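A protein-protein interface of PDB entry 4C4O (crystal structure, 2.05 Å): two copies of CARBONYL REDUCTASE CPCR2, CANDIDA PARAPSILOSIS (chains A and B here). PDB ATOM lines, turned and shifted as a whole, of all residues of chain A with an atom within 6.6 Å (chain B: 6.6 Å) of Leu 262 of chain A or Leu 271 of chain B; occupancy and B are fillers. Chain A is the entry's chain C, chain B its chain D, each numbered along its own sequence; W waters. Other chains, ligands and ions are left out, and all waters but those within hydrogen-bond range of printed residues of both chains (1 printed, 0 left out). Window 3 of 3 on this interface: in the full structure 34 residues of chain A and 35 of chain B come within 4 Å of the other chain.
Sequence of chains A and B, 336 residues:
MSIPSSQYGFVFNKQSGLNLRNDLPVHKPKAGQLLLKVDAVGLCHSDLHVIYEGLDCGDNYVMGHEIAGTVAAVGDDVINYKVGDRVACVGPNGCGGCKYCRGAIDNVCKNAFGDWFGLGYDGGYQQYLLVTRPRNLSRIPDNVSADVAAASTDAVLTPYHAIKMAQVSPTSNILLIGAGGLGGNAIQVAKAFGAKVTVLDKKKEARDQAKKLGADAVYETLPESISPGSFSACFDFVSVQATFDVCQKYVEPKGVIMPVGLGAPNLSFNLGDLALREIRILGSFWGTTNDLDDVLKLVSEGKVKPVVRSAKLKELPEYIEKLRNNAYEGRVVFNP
O of Pro 265 of chain A sits at hydrogen-bond distance from N of Leu 271 of chain B, at 2.9 Å. The backbone carbonyl oxygen (O) of Leu 267 of chain A is in hydrogen-bond range of the backbone NH (N) of Phe 269 of chain B (2.9 Å).
CD1 of Leu 271 of chain B touches CB of Ser 239 of chain A, 3.9 Å away. Pro 259 of chain A touches Leu 271 of chain B. CD2 of Leu 274 of chain B touches CG of Pro 259 of chain A, at 3.9 Å. Gly 261 of chain A touches Leu 271 of chain B. Leu 262 of chain A touches Leu 271 of chain B. Leu 271 of chain B touches Ala 264 of chain A. O of Phe 269 of chain B touches CA of Asn 266 of chain A, at 3.2 Å. Asn 266 of chain A touches Asn 270 of chain B (OD1 to CA, 3.5 Å). CG of Leu 271 of chain B touches CD1 of Leu 267 of chain A, 3.9 Å away. Ala 275 of chain B touches Ser 284 of chain A (O to C, 3.6 Å).
Water W1 lies within hydrogen-bond range of O of Pro 265 of chain A, N of Gly 272 of chain B and OD1 of Asn 270 of chain B.
The side-chain carboxylate (OD1) of Asp 236 of chain A lies within hydrogen-bond range of the backbone NH (N) of Ser 239 of chain A. The side-chain hydroxyl (OG) of Ser 239 of chain A lies within hydrogen-bond range of the backbone carbonyl oxygen (O) of Gly 261 of chain A (3.0 Å). The backbone carbonyl oxygen (O) of Ser 239 of chain A lies within hydrogen-bond range of the backbone NH (N) of Gly 263 of chain A, 3.3 Å away. O of Ser 239 of chain A lies within hydrogen-bond range of N of Ala 264 of chain A, 3.2 Å away. The side-chain amide oxygen of Gln 248 of chain B is in hydrogen-bond range of the backbone NH of Asn 270 of chain B (3.0 Å). The side-chain amide oxygen (OD1) of Asn 270 of chain B lies within hydrogen-bond range of the backbone NH (N) of Gly 272 of chain B, 3.3 Å away.
Of chain B, only Leu 271 comes within 4 Å of Leu 262 of chain A. Of chain A, only Ser 239 (3.9 Å), Pro 259 (3.8 Å), Gly 261 (3.4 Å), Leu 262 (3.9 Å), Ala 264 (3.3 Å), Pro 265 (2.9 Å) and Leu 267 (3.9 Å) come within 4 Å of Leu 271 of chain B. Of the printed residues of chain B, Gly 261 of chain A touches Leu 271. Printed residues of chain B within 4 Å of Pro 259 of chain A: Leu 271 (3.8 Å) and Leu 274 (3.9 Å). Of the printed residues of chain A, Asn 270 of chain B touches Pro 265 (3.7 Å) and Asn 266 (3.5 Å). Of the printed residues of chain B, Ala 264 of chain A touches Leu 271. Val 238 of chain A touches none of the printed residues of chain B. The nearest residue of chain B that does not touch Leu 262 of chain A is Ala 275 of chain B (4.2 Å).
No position is printed for both chains.
Of the 15 printed residues of chain A, 9 touch a printed residue of chain B. Printed residues of chain A that touch a printed residue of chain B: Ser 239, Pro 259, Gly 261, Leu 262, Ala 264, Pro 265, Asn 266, Leu 267 and Ser 284. Hydrophobic or aromatic side chains of chain A that line the printed part of chain B: Pro 259 and Leu 267. Along chain A the printed residues that touch a printed residue of chain B span positions 239 to 284. Printed residues of chain B that touch a printed residue of chain A: Phe 269, Asn 270, Leu 271, Leu 274 and Ala 275. Hydrophobic or aromatic side chains of chain B that line the printed part of chain A: Phe 269, Leu 271 and Leu 274. Among the printed residues, 13 pairs touch across the chains.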
ATOM      1  N   ASP A 236      -6.749  -1.681 -16.747  1.00  0.00           N
ATOM      2  CA  ASP A 236      -5.528  -2.095 -16.024  1.00  0.00           C
ATOM      3  C   ASP A 236      -5.882  -3.202 -15.056  1.00  0.00           C
ATOM      4  O   ASP A 236      -6.510  -2.947 -13.987  1.00  0.00           O
ATOM      5  CB  ASP A 236      -4.983  -0.879 -15.304  1.00  0.00           C
ATOM      6  CG  ASP A 236      -3.606  -1.109 -14.711  1.00  0.00           C
ATOM      7  OD1 ASP A 236      -3.135  -2.271 -14.743  1.00  0.00           O
ATOM      8  OD2 ASP A 236      -3.014  -0.092 -14.292  1.00  0.00           O
ATOM      9  N   PHE A 237      -5.505  -4.439 -15.403  1.00  0.00           N
ATOM     10  CA  PHE A 237      -5.731  -5.573 -14.529  1.00  0.00           C
ATOM     11  C   PHE A 237      -4.569  -5.778 -13.531  1.00  0.00           C
ATOM     12  O   PHE A 237      -4.563  -6.751 -12.790  1.00  0.00           O
ATOM     13  CB  PHE A 237      -6.051  -6.878 -15.326  1.00  0.00           C
ATOM     14  CG  PHE A 237      -7.318  -6.774 -16.144  1.00  0.00           C
ATOM     15  CD1 PHE A 237      -8.572  -6.948 -15.563  1.00  0.00           C
ATOM     16  CD2 PHE A 237      -7.254  -6.347 -17.466  1.00  0.00           C
ATOM     17  CE1 PHE A 237      -9.727  -6.785 -16.313  1.00  0.00           C
ATOM     18  CE2 PHE A 237      -8.415  -6.177 -18.208  1.00  0.00           C
ATOM     19  CZ  PHE A 237      -9.641  -6.369 -17.632  1.00  0.00           C
ATOM     20  N   VAL A 238      -3.608  -4.880 -13.524  1.00  0.00           N
ATOM     21  CA  VAL A 238      -2.490  -4.958 -12.567  1.00  0.00           C
ATOM     22  C   VAL A 238      -2.622  -3.860 -11.498  1.00  0.00           C
ATOM     23  O   VAL A 238      -2.692  -4.143 -10.303  1.00  0.00           O
ATOM     24  CB  VAL A 238      -1.155  -4.803 -13.337  1.00  0.00           C
ATOM     25  CG1 VAL A 238       0.058  -4.705 -12.396  1.00  0.00           C
ATOM     26  CG2 VAL A 238      -0.967  -5.970 -14.343  1.00  0.00           C
ATOM     27  N   SER A 239      -2.713  -2.596 -11.947  1.00  0.00           N
ATOM     28  CA  SER A 239      -2.983  -1.440 -11.083  1.00  0.00           C
ATOM     29  C   SER A 239      -1.866  -1.162 -10.033  1.00  0.00           C
ATOM     30  O   SER A 239      -2.149  -1.066  -8.852  1.00  0.00           O
ATOM     31  CB  SER A 239      -4.340  -1.587 -10.390  1.00  0.00           C
ATOM     32  OG  SER A 239      -5.423  -1.433 -11.314  1.00  0.00           O
ATOM     33  N   VAL A 240      -0.618  -1.059 -10.506  1.00  0.00           N
ATOM     34  CA  VAL A 240       0.451  -0.401  -9.758  1.00  0.00           C
ATOM     35  C   VAL A 240       0.660   0.905 -10.439  1.00  0.00           C
ATOM     36  O   VAL A 240       0.142   1.154 -11.551  1.00  0.00           O
ATOM     37  CB  VAL A 240       1.770  -1.233  -9.703  1.00  0.00           C
ATOM     38  CG1 VAL A 240       1.504  -2.550  -9.022  1.00  0.00           C
ATOM     39  CG2 VAL A 240       2.362  -1.473 -11.095  1.00  0.00           C
ATOM     40  N   PRO A 259      -9.256   1.046 -13.586  1.00  0.00           N
ATOM     41  CA  PRO A 259      -8.266   0.294 -12.763  1.00  0.00           C
ATOM     42  C   PRO A 259      -8.960  -0.869 -12.068  1.00  0.00           C
ATOM     43  O   PRO A 259      -9.423  -0.731 -10.939  1.00  0.00           O
ATOM     44  CB  PRO A 259      -7.792   1.353 -11.750  1.00  0.00           C
ATOM     45  CG  PRO A 259      -8.942   2.265 -11.608  1.00  0.00           C
ATOM     46  CD  PRO A 259      -9.756   2.242 -12.893  1.00  0.00           C
ATOM     47  N   VAL A 260      -8.974  -2.015 -12.730  1.00  0.00           N
ATOM     48  CA  VAL A 260      -9.714  -3.150 -12.300  1.00  0.00           C
ATOM     49  C   VAL A 260      -8.870  -4.027 -11.355  1.00  0.00           C
ATOM     50  O   VAL A 260      -9.402  -4.633 -10.422  1.00  0.00           O
ATOM     51  CB  VAL A 260     -10.192  -3.990 -13.503  1.00  0.00           C
ATOM     52  CG1 VAL A 260     -10.923  -5.229 -13.012  1.00  0.00           C
ATOM     53  CG2 VAL A 260     -11.172  -3.209 -14.350  1.00  0.00           C
ATOM     54  N   GLY A 261      -7.572  -4.072 -11.569  1.00  0.00           N
ATOM     55  CA  GLY A 261      -6.658  -4.749 -10.628  1.00  0.00           C
ATOM     56  C   GLY A 261      -6.488  -4.047  -9.299  1.00  0.00           C
ATOM     57  O   GLY A 261      -6.856  -2.885  -9.143  1.00  0.00           O
ATOM     58  N   LEU A 262      -5.907  -4.749  -8.339  1.00  0.00           N
ATOM     59  CA  LEU A 262      -5.715  -4.205  -6.993  1.00  0.00           C
ATOM     60  C   LEU A 262      -4.238  -4.337  -6.546  1.00  0.00           C
ATOM     61  O   LEU A 262      -3.959  -4.897  -5.537  1.00  0.00           O
ATOM     62  CB  LEU A 262      -6.681  -4.859  -6.011  1.00  0.00           C
ATOM     63  CG  LEU A 262      -8.187  -4.735  -6.458  1.00  0.00           C
ATOM     64  CD1 LEU A 262      -9.199  -5.574  -5.673  1.00  0.00           C
ATOM     65  CD2 LEU A 262      -8.703  -3.293  -6.502  1.00  0.00           C
ATOM     66  N   GLY A 263      -3.308  -3.781  -7.304  1.00  0.00           N
ATOM     67  CA  GLY A 263      -1.879  -3.996  -7.063  1.00  0.00           C
ATOM     68  C   GLY A 263      -1.215  -2.976  -6.120  1.00  0.00           C
ATOM     69  O   GLY A 263      -0.076  -3.154  -5.697  1.00  0.00           O
ATOM     70  N   ALA A 264      -1.917  -1.892  -5.821  1.00  0.00           N
ATOM     71  CA  ALA A 264      -1.486  -0.910  -4.864  1.00  0.00           C
ATOM     72  C   ALA A 264      -2.680  -0.336  -4.132  1.00  0.00           C
ATOM     73  O   ALA A 264      -3.795  -0.335  -4.657  1.00  0.00           O
ATOM     74  CB  ALA A 264      -0.696   0.173  -5.548  1.00  0.00           C
ATOM     75  N   PRO A 265      -2.458   0.156  -2.912  1.00  0.00           N
ATOM     76  CA  PRO A 265      -3.593   0.617  -2.144  1.00  0.00           C
ATOM     77  C   PRO A 265      -4.076   1.952  -2.612  1.00  0.00           C
ATOM     78  O   PRO A 265      -5.239   2.271  -2.389  1.00  0.00           O
ATOM     79  CB  PRO A 265      -3.056   0.686  -0.691  1.00  0.00           C
ATOM     80  CG  PRO A 265      -1.555   0.732  -0.841  1.00  0.00           C
ATOM     81  CD  PRO A 265      -1.249  -0.063  -2.077  1.00  0.00           C
ATOM     82  N   ASN A 266      -3.175   2.740  -3.208  1.00  0.00           N
ATOM     83  CA  ASN A 266      -3.432   4.102  -3.664  1.00  0.00           C
ATOM     84  C   ASN A 266      -2.730   4.315  -5.002  1.00  0.00           C
ATOM     85  O   ASN A 266      -1.729   3.678  -5.263  1.00  0.00           O
ATOM     86  CB  ASN A 266      -2.896   5.152  -2.688  1.00  0.00           C
ATOM     87  CG  ASN A 266      -3.533   5.012  -1.328  1.00  0.00           C
ATOM     88  OD1 ASN A 266      -4.496   5.718  -0.980  1.00  0.00           O
ATOM     89  ND2 ASN A 266      -3.068   4.075  -0.594  1.00  0.00           N
ATOM     90  N   LEU A 267      -3.296   5.155  -5.869  1.00  0.00           N
ATOM     91  CA  LEU A 267      -2.655   5.477  -7.125  1.00  0.00           C
ATOM     92  C   LEU A 267      -2.790   6.909  -7.340  1.00  0.00           C
ATOM     93  O   LEU A 267      -3.762   7.513  -6.901  1.00  0.00           O
ATOM     94  CB  LEU A 267      -3.372   4.744  -8.317  1.00  0.00           C
ATOM     95  CG  LEU A 267      -3.284   3.207  -8.397  1.00  0.00           C
ATOM     96  CD1 LEU A 267      -4.210   2.676  -9.511  1.00  0.00           C
ATOM     97  CD2 LEU A 267      -1.872   2.757  -8.687  1.00  0.00           C
ATOM     98  N   SER A 284     -14.906  -0.095 -10.776  1.00  0.00           N
ATOM     99  CA  SER A 284     -15.658  -1.237 -11.189  1.00  0.00           C
ATOM    100  C   SER A 284     -15.456  -2.362 -10.198  1.00  0.00           C
ATOM    101  O   SER A 284     -14.327  -2.696  -9.861  1.00  0.00           O
ATOM    102  CB  SER A 284     -15.187  -1.699 -12.584  1.00  0.00           C
ATOM    103  OG  SER A 284     -16.194  -2.537 -13.131  1.00  0.00           O
ATOM    104  N   GLN B 248     -13.400  11.998  -1.431  1.00  0.00           N
ATOM    105  CA  GLN B 248     -13.438  10.572  -1.509  1.00  0.00           C
ATOM    106  C   GLN B 248     -14.107   9.935  -0.299  1.00  0.00           C
ATOM    107  O   GLN B 248     -14.768   8.940  -0.421  1.00  0.00           O
ATOM    108  CB  GLN B 248     -12.047   9.942  -1.808  1.00  0.00           C
ATOM    109  CG  GLN B 248     -12.212   8.454  -2.004  1.00  0.00           C
ATOM    110  CD  GLN B 248     -11.079   7.751  -2.683  1.00  0.00           C
ATOM    111  OE1 GLN B 248      -9.961   8.260  -2.806  1.00  0.00           O
ATOM    112  NE2 GLN B 248     -11.355   6.510  -3.102  1.00  0.00           N
ATOM    113  N   PHE B 269      -5.754   8.676  -5.208  1.00  0.00           N
ATOM    114  CA  PHE B 269      -6.990   8.115  -4.682  1.00  0.00           C
ATOM    115  C   PHE B 269      -6.761   6.781  -4.126  1.00  0.00           C
ATOM    116  O   PHE B 269      -5.810   6.098  -4.521  1.00  0.00           O
ATOM    117  CB  PHE B 269      -8.031   8.071  -5.833  1.00  0.00           C
ATOM    118  CG  PHE B 269      -7.650   7.180  -7.004  1.00  0.00           C
ATOM    119  CD1 PHE B 269      -7.953   5.831  -6.991  1.00  0.00           C
ATOM    120  CD2 PHE B 269      -7.075   7.696  -8.116  1.00  0.00           C
ATOM    121  CE1 PHE B 269      -7.679   5.031  -8.087  1.00  0.00           C
ATOM    122  CE2 PHE B 269      -6.757   6.915  -9.212  1.00  0.00           C
ATOM    123  CZ  PHE B 269      -7.030   5.570  -9.182  1.00  0.00           C
ATOM    124  N   ASN B 270      -7.607   6.386  -3.172  1.00  0.00           N
ATOM    125  CA  ASN B 270      -7.581   5.098  -2.591  1.00  0.00           C
ATOM    126  C   ASN B 270      -8.241   4.121  -3.550  1.00  0.00           C
ATOM    127  O   ASN B 270      -9.418   4.253  -3.826  1.00  0.00           O
ATOM    128  CB  ASN B 270      -8.375   5.148  -1.272  1.00  0.00           C
ATOM    129  CG  ASN B 270      -8.414   3.828  -0.546  1.00  0.00           C
ATOM    130  OD1 ASN B 270      -8.798   2.803  -1.067  1.00  0.00           O
ATOM    131  ND2 ASN B 270      -7.952   3.847   0.685  1.00  0.00           N
ATOM    132  N   LEU B 271      -7.505   3.101  -3.991  1.00  0.00           N
ATOM    133  CA  LEU B 271      -7.961   2.247  -5.114  1.00  0.00           C
ATOM    134  C   LEU B 271      -9.031   1.284  -4.643  1.00  0.00           C
ATOM    135  O   LEU B 271     -10.032   1.080  -5.320  1.00  0.00           O
ATOM    136  CB  LEU B 271      -6.792   1.444  -5.631  1.00  0.00           C
ATOM    137  CG  LEU B 271      -6.731   0.934  -7.052  1.00  0.00           C
ATOM    138  CD1 LEU B 271      -5.943  -0.344  -7.107  1.00  0.00           C
ATOM    139  CD2 LEU B 271      -8.028   0.868  -7.810  1.00  0.00           C
ATOM    140  N   GLY B 272      -8.789   0.616  -3.507  1.00  0.00           N
ATOM    141  CA  GLY B 272      -9.768  -0.311  -2.975  1.00  0.00           C
ATOM    142  C   GLY B 272     -11.115   0.342  -2.795  1.00  0.00           C
ATOM    143  O   GLY B 272     -12.152  -0.251  -3.099  1.00  0.00           O
ATOM    144  N   ASP B 273     -11.118   1.570  -2.291  1.00  0.00           N
ATOM    145  CA  ASP B 273     -12.336   2.286  -2.060  1.00  0.00           C
ATOM    146  C   ASP B 273     -13.004   2.689  -3.442  1.00  0.00           C
ATOM    147  O   ASP B 273     -14.205   2.546  -3.612  1.00  0.00           O
ATOM    148  CB  ASP B 273     -12.065   3.527  -1.279  1.00  0.00           C
ATOM    149  CG  ASP B 273     -13.326   4.347  -1.051  1.00  0.00           C
ATOM    150  OD1 ASP B 273     -14.131   3.941  -0.198  1.00  0.00           O
ATOM    151  OD2 ASP B 273     -13.563   5.356  -1.731  1.00  0.00           O
ATOM    152  N   LEU B 274     -12.209   3.206  -4.372  1.00  0.00           N
ATOM    153  CA  LEU B 274     -12.727   3.607  -5.669  1.00  0.00           C
ATOM    154  C   LEU B 274     -13.362   2.417  -6.429  1.00  0.00           C
ATOM    155  O   LEU B 274     -14.466   2.522  -6.940  1.00  0.00           O
ATOM    156  CB  LEU B 274     -11.647   4.280  -6.489  1.00  0.00           C
ATOM    157  CG  LEU B 274     -12.089   4.631  -7.899  1.00  0.00           C
ATOM    158  CD1 LEU B 274     -11.846   6.042  -8.204  1.00  0.00           C
ATOM    159  CD2 LEU B 274     -11.416   3.757  -8.954  1.00  0.00           C
ATOM    160  N   ALA B 275     -12.733   1.269  -6.330  1.00  0.00           N
ATOM    161  CA  ALA B 275     -13.206   0.071  -6.970  1.00  0.00           C
ATOM    162  C   ALA B 275     -14.434  -0.489  -6.302  1.00  0.00           C
ATOM    163  O   ALA B 275     -15.485  -0.706  -6.949  1.00  0.00           O
ATOM    164  CB  ALA B 275     -12.100  -0.964  -7.023  1.00  0.00           C
ATOM    165  N   LEU B 276     -14.325  -0.713  -5.015  1.00  0.00           N
ATOM    166  CA  LEU B 276     -15.420  -1.327  -4.266  1.00  0.00           C
ATOM    167  C   LEU B 276     -16.719  -0.536  -4.285  1.00  0.00           C
ATOM    168  O   LEU B 276     -17.796  -1.100  -4.419  1.00  0.00           O
ATOM    169  CB  LEU B 276     -14.993  -1.503  -2.814  1.00  0.00           C
ATOM    170  CG  LEU B 276     -16.029  -2.368  -2.062  1.00  0.00           C
HETATM  171  O   HOH W   1      -6.917   0.464  -1.389  1.00  0.00           O
